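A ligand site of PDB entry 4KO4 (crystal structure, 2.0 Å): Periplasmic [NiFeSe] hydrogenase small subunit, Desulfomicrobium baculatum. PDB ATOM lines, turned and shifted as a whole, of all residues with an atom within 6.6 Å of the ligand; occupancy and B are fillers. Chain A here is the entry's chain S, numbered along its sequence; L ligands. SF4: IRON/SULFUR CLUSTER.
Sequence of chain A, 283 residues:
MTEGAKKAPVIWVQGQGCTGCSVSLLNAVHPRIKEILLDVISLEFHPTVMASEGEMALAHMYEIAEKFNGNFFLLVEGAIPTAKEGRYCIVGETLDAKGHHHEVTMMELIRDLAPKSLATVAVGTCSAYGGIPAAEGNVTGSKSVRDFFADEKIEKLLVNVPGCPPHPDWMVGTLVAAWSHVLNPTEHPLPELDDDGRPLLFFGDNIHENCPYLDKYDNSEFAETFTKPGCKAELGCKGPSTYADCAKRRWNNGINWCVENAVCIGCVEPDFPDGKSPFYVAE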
ATOM      1  N   ILE A 207      12.574   4.341  29.723  1.00  0.00           N
ATOM      2  CA  ILE A 207      12.565   3.176  28.826  1.00  0.00           C
ATOM      3  C   ILE A 207      13.039   1.910  29.549  1.00  0.00           C
ATOM      4  O   ILE A 207      12.340   0.896  29.555  1.00  0.00           O
ATOM      5  CB  ILE A 207      13.449   3.439  27.574  1.00  0.00           C
ATOM      6  CG1 ILE A 207      12.887   4.626  26.776  1.00  0.00           C
ATOM      7  CG2 ILE A 207      13.661   2.127  26.758  1.00  0.00           C
ATOM      8  CD1 ILE A 207      12.114   4.298  25.525  1.00  0.00           C
ATOM      9  N   HIS A 208      14.212   1.991  30.174  1.00  0.00           N
ATOM     10  CA  HIS A 208      14.836   0.853  30.859  1.00  0.00           C
ATOM     11  C   HIS A 208      13.933   0.266  31.950  1.00  0.00           C
ATOM     12  O   HIS A 208      13.703  -0.949  32.002  1.00  0.00           O
ATOM     13  CB  HIS A 208      16.214   1.303  31.368  1.00  0.00           C
ATOM     14  CG  HIS A 208      16.956   0.276  32.160  1.00  0.00           C
ATOM     15  ND1 HIS A 208      17.618  -0.787  31.585  1.00  0.00           N
ATOM     16  CD2 HIS A 208      17.196   0.202  33.494  1.00  0.00           C
ATOM     17  CE1 HIS A 208      18.212  -1.494  32.535  1.00  0.00           C
ATOM     18  NE2 HIS A 208      17.969  -0.921  33.699  1.00  0.00           N
ATOM     19  N   GLU A 209      13.380   1.124  32.806  1.00  0.00           N
ATOM     20  CA  GLU A 209      12.516   0.658  33.897  1.00  0.00           C
ATOM     21  C   GLU A 209      11.317  -0.099  33.360  1.00  0.00           C
ATOM     22  O   GLU A 209      10.775  -0.977  34.036  1.00  0.00           O
ATOM     23  CB  GLU A 209      12.065   1.822  34.789  1.00  0.00           C
ATOM     24  CG  GLU A 209      13.208   2.462  35.586  1.00  0.00           C
ATOM     25  CD  GLU A 209      12.764   3.680  36.401  1.00  0.00           C
ATOM     26  OE1 GLU A 209      11.544   3.886  36.610  1.00  0.00           O
ATOM     27  OE2 GLU A 209      13.640   4.444  36.829  1.00  0.00           O
ATOM     28  N   CYS A 211      11.304  -1.786  30.327  1.00  0.00           N
ATOM     29  CA  CYS A 211      11.762  -2.606  29.208  1.00  0.00           C
ATOM     30  C   CYS A 211      11.502  -4.090  29.435  1.00  0.00           C
ATOM     31  O   CYS A 211      11.765  -4.608  30.529  1.00  0.00           O
ATOM     32  CB  CYS A 211      13.247  -2.373  28.970  1.00  0.00           C
ATOM     33  SG  CYS A 211      13.906  -3.269  27.562  1.00  0.00           S
ATOM     34  N   PRO A 212      11.018  -4.796  28.398  1.00  0.00           N
ATOM     35  CA  PRO A 212      10.813  -6.243  28.537  1.00  0.00           C
ATOM     36  C   PRO A 212      12.106  -7.055  28.724  1.00  0.00           C
ATOM     37  O   PRO A 212      12.050  -8.235  29.073  1.00  0.00           O
ATOM     38  CB  PRO A 212      10.105  -6.635  27.232  1.00  0.00           C
ATOM     39  CG  PRO A 212      10.448  -5.551  26.249  1.00  0.00           C
ATOM     40  CD  PRO A 212      10.604  -4.294  27.064  1.00  0.00           C
ATOM     41  N   TYR A 213      13.262  -6.437  28.475  1.00  0.00           N
ATOM     42  CA  TYR A 213      14.554  -7.118  28.670  1.00  0.00           C
ATOM     43  C   TYR A 213      15.100  -6.922  30.091  1.00  0.00           C
ATOM     44  O   TYR A 213      16.210  -7.379  30.377  1.00  0.00           O
ATOM     45  CB  TYR A 213      15.601  -6.619  27.675  1.00  0.00           C
ATOM     46  CG  TYR A 213      15.381  -7.020  26.231  1.00  0.00           C
ATOM     47  CD1 TYR A 213      14.557  -6.253  25.408  1.00  0.00           C
ATOM     48  CD2 TYR A 213      16.036  -8.132  25.679  1.00  0.00           C
ATOM     49  CE1 TYR A 213      14.343  -6.609  24.062  1.00  0.00           C
ATOM     50  CE2 TYR A 213      15.838  -8.485  24.315  1.00  0.00           C
ATOM     51  CZ  TYR A 213      14.993  -7.719  23.533  1.00  0.00           C
ATOM     52  OH  TYR A 213      14.775  -8.038  22.213  1.00  0.00           O
ATOM     53  N   LEU A 214      14.360  -6.230  30.955  1.00  0.00           N
ATOM     54  CA  LEU A 214      14.883  -5.882  32.274  1.00  0.00           C
ATOM     55  C   LEU A 214      15.250  -7.126  33.100  1.00  0.00           C
ATOM     56  O   LEU A 214      16.240  -7.107  33.835  1.00  0.00           O
ATOM     57  CB  LEU A 214      13.936  -4.946  33.045  1.00  0.00           C
ATOM     58  CG  LEU A 214      14.502  -4.305  34.326  1.00  0.00           C
ATOM     59  CD1 LEU A 214      15.691  -3.385  34.034  1.00  0.00           C
ATOM     60  CD2 LEU A 214      13.401  -3.523  35.015  1.00  0.00           C
ATOM     61  N   ASP A 215      14.461  -8.199  32.968  1.00  0.00           N
ATOM     62  CA  ASP A 215      14.785  -9.453  33.670  1.00  0.00           C
ATOM     63  C   ASP A 215      16.160  -9.991  33.233  1.00  0.00           C
ATOM     64  O   ASP A 215      16.955 -10.451  34.063  1.00  0.00           O
ATOM     65  CB  ASP A 215      13.675 -10.511  33.483  1.00  0.00           C
ATOM     66  CG  ASP A 215      13.434 -10.903  32.005  1.00  0.00           C
ATOM     67  OD1 ASP A 215      13.727 -10.117  31.062  1.00  0.00           O
ATOM     68  OD2 ASP A 215      12.923 -12.023  31.792  1.00  0.00           O
ATOM     69  N   LYS A 216      16.454  -9.886  31.949  1.00  0.00           N
ATOM     70  CA  LYS A 216      17.737 -10.323  31.405  1.00  0.00           C
ATOM     71  C   LYS A 216      18.875  -9.447  31.910  1.00  0.00           C
ATOM     72  O   LYS A 216      19.918  -9.952  32.333  1.00  0.00           O
ATOM     73  CB  LYS A 216      17.686 -10.377  29.882  1.00  0.00           C
ATOM     74  CG  LYS A 216      16.714 -11.422  29.350  1.00  0.00           C
ATOM     75  CD  LYS A 216      16.601 -11.393  27.827  1.00  0.00           C
ATOM     76  CE  LYS A 216      15.318 -12.068  27.330  1.00  0.00           C
ATOM     77  NZ  LYS A 216      14.926 -13.250  28.144  1.00  0.00           N
ATOM     78  N   TYR A 217      18.666  -8.128  31.871  1.00  0.00           N
ATOM     79  CA  TYR A 217      19.610  -7.185  32.443  1.00  0.00           C
ATOM     80  C   TYR A 217      19.934  -7.551  33.901  1.00  0.00           C
ATOM     81  O   TYR A 217      21.111  -7.578  34.300  1.00  0.00           O
ATOM     82  CB  TYR A 217      19.024  -5.754  32.357  1.00  0.00           C
ATOM     83  CG  TYR A 217      19.869  -4.695  33.022  1.00  0.00           C
ATOM     84  CD1 TYR A 217      19.711  -4.399  34.376  1.00  0.00           C
ATOM     85  CD2 TYR A 217      20.816  -3.953  32.291  1.00  0.00           C
ATOM     86  CE1 TYR A 217      20.482  -3.414  35.015  1.00  0.00           C
ATOM     87  CE2 TYR A 217      21.586  -2.954  32.921  1.00  0.00           C
ATOM     88  CZ  TYR A 217      21.404  -2.696  34.272  1.00  0.00           C
ATOM     89  OH  TYR A 217      22.152  -1.729  34.888  1.00  0.00           O
ATOM     90  N   PHE A 222      23.508 -10.511  28.686  1.00  0.00           N
ATOM     91  CA  PHE A 222      23.691  -9.469  27.683  1.00  0.00           C
ATOM     92  C   PHE A 222      23.994 -10.046  26.306  1.00  0.00           C
ATOM     93  O   PHE A 222      24.848 -10.922  26.159  1.00  0.00           O
ATOM     94  CB  PHE A 222      24.809  -8.513  28.091  1.00  0.00           C
ATOM     95  CG  PHE A 222      24.566  -7.849  29.424  1.00  0.00           C
ATOM     96  CD1 PHE A 222      23.594  -6.857  29.553  1.00  0.00           C
ATOM     97  CD2 PHE A 222      25.299  -8.231  30.537  1.00  0.00           C
ATOM     98  CE1 PHE A 222      23.363  -6.249  30.779  1.00  0.00           C
ATOM     99  CE2 PHE A 222      25.085  -7.625  31.767  1.00  0.00           C
ATOM    100  CZ  PHE A 222      24.100  -6.631  31.901  1.00  0.00           C
ATOM    101  N   GLY A 230      19.503 -11.679  24.825  1.00  0.00           N
ATOM    102  CA  GLY A 230      19.914 -10.927  25.994  1.00  0.00           C
ATOM    103  C   GLY A 230      19.593  -9.444  25.915  1.00  0.00           C
ATOM    104  O   GLY A 230      19.189  -8.920  24.872  1.00  0.00           O
ATOM    105  N   CYS A 231      19.746  -8.767  27.052  1.00  0.00           N
ATOM    106  CA  CYS A 231      19.640  -7.320  27.116  1.00  0.00           C
ATOM    107  C   CYS A 231      20.641  -6.661  26.138  1.00  0.00           C
ATOM    108  O   CYS A 231      21.732  -7.211  25.882  1.00  0.00           O
ATOM    109  CB  CYS A 231      19.867  -6.869  28.570  1.00  0.00           C
ATOM    110  SG  CYS A 231      20.334  -5.156  28.822  1.00  0.00           S
ATOM    111  N   LYS A 232      20.287  -5.496  25.620  1.00  0.00           N
ATOM    112  CA  LYS A 232      21.090  -4.786  24.601  1.00  0.00           C
ATOM    113  C   LYS A 232      22.125  -3.802  25.178  1.00  0.00           C
ATOM    114  O   LYS A 232      22.767  -3.083  24.428  1.00  0.00           O
ATOM    115  CB  LYS A 232      20.152  -4.015  23.664  1.00  0.00           C
ATOM    116  CG  LYS A 232      19.005  -4.835  23.078  1.00  0.00           C
ATOM    117  CD  LYS A 232      19.511  -6.050  22.259  1.00  0.00           C
ATOM    118  CE  LYS A 232      18.374  -6.712  21.469  1.00  0.00           C
ATOM    119  NZ  LYS A 232      17.969  -5.904  20.298  1.00  0.00           N
ATOM    120  N   ALA A 233      22.279  -3.759  26.513  1.00  0.00           N
ATOM    121  CA  ALA A 233      23.134  -2.761  27.160  1.00  0.00           C
ATOM    122  C   ALA A 233      24.558  -2.721  26.610  1.00  0.00           C
ATOM    123  O   ALA A 233      25.104  -1.635  26.391  1.00  0.00           O
ATOM    124  CB  ALA A 233      23.178  -2.979  28.683  1.00  0.00           C
ATOM    125  N   GLU A 234      25.170  -3.893  26.391  1.00  0.00           N
ATOM    126  CA  GLU A 234      26.556  -3.929  25.931  1.00  0.00           C
ATOM    127  C   GLU A 234      26.699  -3.515  24.455  1.00  0.00           C
ATOM    128  O   GLU A 234      27.806  -3.211  23.993  1.00  0.00           O
ATOM    129  CB  GLU A 234      27.196  -5.301  26.160  1.00  0.00           C
ATOM    130  CG  GLU A 234      27.385  -5.678  27.622  1.00  0.00           C
ATOM    131  CD  GLU A 234      27.989  -7.052  27.790  1.00  0.00           C
ATOM    132  OE1 GLU A 234      28.199  -7.464  28.946  1.00  0.00           O
ATOM    133  OE2 GLU A 234      28.235  -7.757  26.782  1.00  0.00           O
ATOM    134  N   CYS A 237      22.816   0.304  24.160  1.00  0.00           N
ATOM    135  CA  CYS A 237      21.460   0.762  24.497  1.00  0.00           C
ATOM    136  C   CYS A 237      21.438   1.928  25.484  1.00  0.00           C
ATOM    137  O   CYS A 237      22.042   1.829  26.569  1.00  0.00           O
ATOM    138  CB  CYS A 237      20.614  -0.401  25.030  1.00  0.00           C
ATOM    139  SG  CYS A 237      18.869   0.025  25.220  1.00  0.00           S
ATOM    140  N   LYS A 238      20.753   3.016  25.107  1.00  0.00           N
ATOM    141  CA  LYS A 238      20.621   4.199  25.980  1.00  0.00           C
ATOM    142  C   LYS A 238      19.271   4.244  26.709  1.00  0.00           C
ATOM    143  O   LYS A 238      18.905   5.267  27.294  1.00  0.00           O
ATOM    144  CB  LYS A 238      20.871   5.501  25.202  1.00  0.00           C
ATOM    145  CG  LYS A 238      22.210   5.515  24.458  1.00  0.00           C
ATOM    146  CD  LYS A 238      23.386   5.239  25.403  1.00  0.00           C
ATOM    147  CE  LYS A 238      24.748   5.482  24.748  1.00  0.00           C
ATOM    148  NZ  LYS A 238      24.916   4.740  23.477  1.00  0.00           N
ATOM    149  N   GLY A 239      18.552   3.119  26.718  1.00  0.00           N
ATOM    150  CA  GLY A 239      17.308   3.010  27.491  1.00  0.00           C
ATOM    151  C   GLY A 239      17.417   3.490  28.933  1.00  0.00           C
ATOM    152  O   GLY A 239      16.498   4.131  29.425  1.00  0.00           O
ATOM    153  N   PRO A 240      18.546   3.185  29.613  1.00  0.00           N
ATOM    154  CA  PRO A 240      18.708   3.632  30.997  1.00  0.00           C
ATOM    155  C   PRO A 240      18.594   5.143  31.221  1.00  0.00           C
ATOM    156  O   PRO A 240      18.132   5.552  32.288  1.00  0.00           O
ATOM    157  CB  PRO A 240      20.100   3.103  31.363  1.00  0.00           C
ATOM    158  CG  PRO A 240      20.177   1.812  30.608  1.00  0.00           C
ATOM    159  CD  PRO A 240      19.609   2.219  29.237  1.00  0.00           C
ATOM    160  N   TRP A 257      10.131  -2.088  17.568  1.00  0.00           N
ATOM    161  CA  TRP A 257      10.701  -0.879  18.187  1.00  0.00           C
ATOM    162  C   TRP A 257      12.212  -0.999  18.302  1.00  0.00           C
ATOM    163  O   TRP A 257      12.764  -2.081  18.103  1.00  0.00           O
ATOM    164  CB  TRP A 257      10.067  -0.544  19.534  1.00  0.00           C
ATOM    165  CG  TRP A 257      10.365  -1.491  20.668  1.00  0.00           C
ATOM    166  CD1 TRP A 257      10.155  -2.847  20.704  1.00  0.00           C
ATOM    167  CD2 TRP A 257      10.853  -1.123  21.970  1.00  0.00           C
ATOM    168  NE1 TRP A 257      10.488  -3.344  21.943  1.00  0.00           N
ATOM    169  CE2 TRP A 257      10.941  -2.324  22.735  1.00  0.00           C
ATOM    170  CE3 TRP A 257      11.238   0.091  22.561  1.00  0.00           C
ATOM    171  CZ2 TRP A 257      11.391  -2.329  24.068  1.00  0.00           C
ATOM    172  CZ3 TRP A 257      11.690   0.078  23.882  1.00  0.00           C
ATOM    173  CH2 TRP A 257      11.770  -1.130  24.618  1.00  0.00           C
ATOM    174  N   VAL A 259      14.564  -1.048  20.599  1.00  0.00           N
ATOM    175  CA  VAL A 259      15.216  -1.945  21.536  1.00  0.00           C
ATOM    176  C   VAL A 259      15.088  -3.396  21.115  1.00  0.00           C
ATOM    177  O   VAL A 259      16.082  -4.113  21.155  1.00  0.00           O
ATOM    178  CB  VAL A 259      14.730  -1.699  22.988  1.00  0.00           C
ATOM    179  CG1 VAL A 259      15.275  -2.786  23.929  1.00  0.00           C
ATOM    180  CG2 VAL A 259      15.167  -0.305  23.456  1.00  0.00           C
ATOM    181  N   ALA A 262      17.279  -3.565  17.864  1.00  0.00           N
ATOM    182  CA  ALA A 262      18.673  -3.141  17.916  1.00  0.00           C
ATOM    183  C   ALA A 262      18.976  -2.505  19.280  1.00  0.00           C
ATOM    184  O   ALA A 262      19.082  -3.227  20.258  1.00  0.00           O
ATOM    185  CB  ALA A 262      19.016  -2.177  16.741  1.00  0.00           C
ATOM    186  N   VAL A 263      19.105  -1.175  19.322  1.00  0.00           N
ATOM    187  CA  VAL A 263      19.323  -0.434  20.576  1.00  0.00           C
ATOM    188  C   VAL A 263      18.497   0.850  20.567  1.00  0.00           C
ATOM    189  O   VAL A 263      18.146   1.378  19.501  1.00  0.00           O
ATOM    190  CB  VAL A 263      20.818  -0.038  20.757  1.00  0.00           C
ATOM    191  CG1 VAL A 263      21.733  -1.272  21.047  1.00  0.00           C
ATOM    192  CG2 VAL A 263      21.325   0.771  19.546  1.00  0.00           C
ATOM    193  N   CYS A 264      18.195   1.363  21.766  1.00  0.00           N
ATOM    194  CA  CYS A 264      17.698   2.741  21.901  1.00  0.00           C
ATOM    195  C   CYS A 264      18.890   3.681  21.783  1.00  0.00           C
ATOM    196  O   CYS A 264      19.955   3.415  22.372  1.00  0.00           O
ATOM    197  CB  CYS A 264      16.985   2.926  23.264  1.00  0.00           C
ATOM    198  SG  CYS A 264      16.445   4.636  23.610  1.00  0.00           S
HETATM  199 FE1  SF4 L   1      18.639  -3.692  28.451  1.00  0.00          FE
HETATM  200 FE2  SF4 L   1      16.129  -2.831  27.905  1.00  0.00          FE
HETATM  201 FE3  SF4 L   1      17.663  -1.521  29.635  1.00  0.00          FE
HETATM  202 FE4  SF4 L   1      18.233  -1.399  26.928  1.00  0.00          FE
HETATM  203  S1  SF4 L   1      16.399  -0.540  27.988  1.00  0.00           S
HETATM  204  S2  SF4 L   1      19.721  -1.665  28.633  1.00  0.00           S
HETATM  205  S3  SF4 L   1      17.661  -3.584  26.393  1.00  0.00           S
HETATM  206  S4  SF4 L   1      16.894  -3.658  29.900  1.00  0.00           S
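FE1 of the ligand is bound by SG of Cys 231. An iron atom (FE4) of the ligand is bound by the side-chain sulfur of Cys 237 (2.3 Å). A sulfur (S3) of the ligand sits close to the backbone NH of Lys 232, 3.3 Å away. S4 of the ligand lies close to N of Leu 214. FE3 of the ligand is bound by ND1 of His 208, at 2.1 Å. An iron atom (FE2) of the ligand is bound by the side-chain sulfur (SG) of Cys 211 (2.3 Å).
The side-chain amino group (NZ) of Lys 232 sits at hydrogen-bond distance from the backbone carbonyl oxygen (O) of Val 259 (2.7 Å). SG of Cys 231 lies close to N of Ala 233 (3.3 Å). O of Lys 232 lies within hydrogen-bond range of N of Cys 237. SG of Cys 211 sits close to N of Tyr 213 (3.4 Å). The backbone NH (N) of His 208 sits at hydrogen-bond distance from the backbone carbonyl oxygen (O) of Gly 239 (3.2 Å). N of Cys 264 lies close to SG of Cys 237 (3.8 Å). The backbone NH (N) of Gly 239 sits close to the side-chain sulfur (SG) of Cys 237, 3.5 Å away. The side-chain amino group (NZ) of Lys 232 is in hydrogen-bond range of the backbone carbonyl oxygen (O) of Ala 262 (2.9 Å).
Tyr 213 touches the ligand. Tyr 217 touches the ligand. CB of Ala 233 touches S2 of the ligand, at 3.7 Å. Gly 239 touches the ligand. Pro 240 touches the ligand (CD to S2, 3.9 Å). Val 259 touches the ligand. Hydrophobic or aromatic side chains that line the ligand: His 208, Tyr 213, Tyr 217, Ala 233, Pro 240 and Val 259. Within 4 Å of the ligand: His 208, Cys 211, Tyr 213, Leu 214, Tyr 217, Cys 231, Lys 232, Ala 233, Cys 237, Gly 239, Pro 240 and Val 259.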
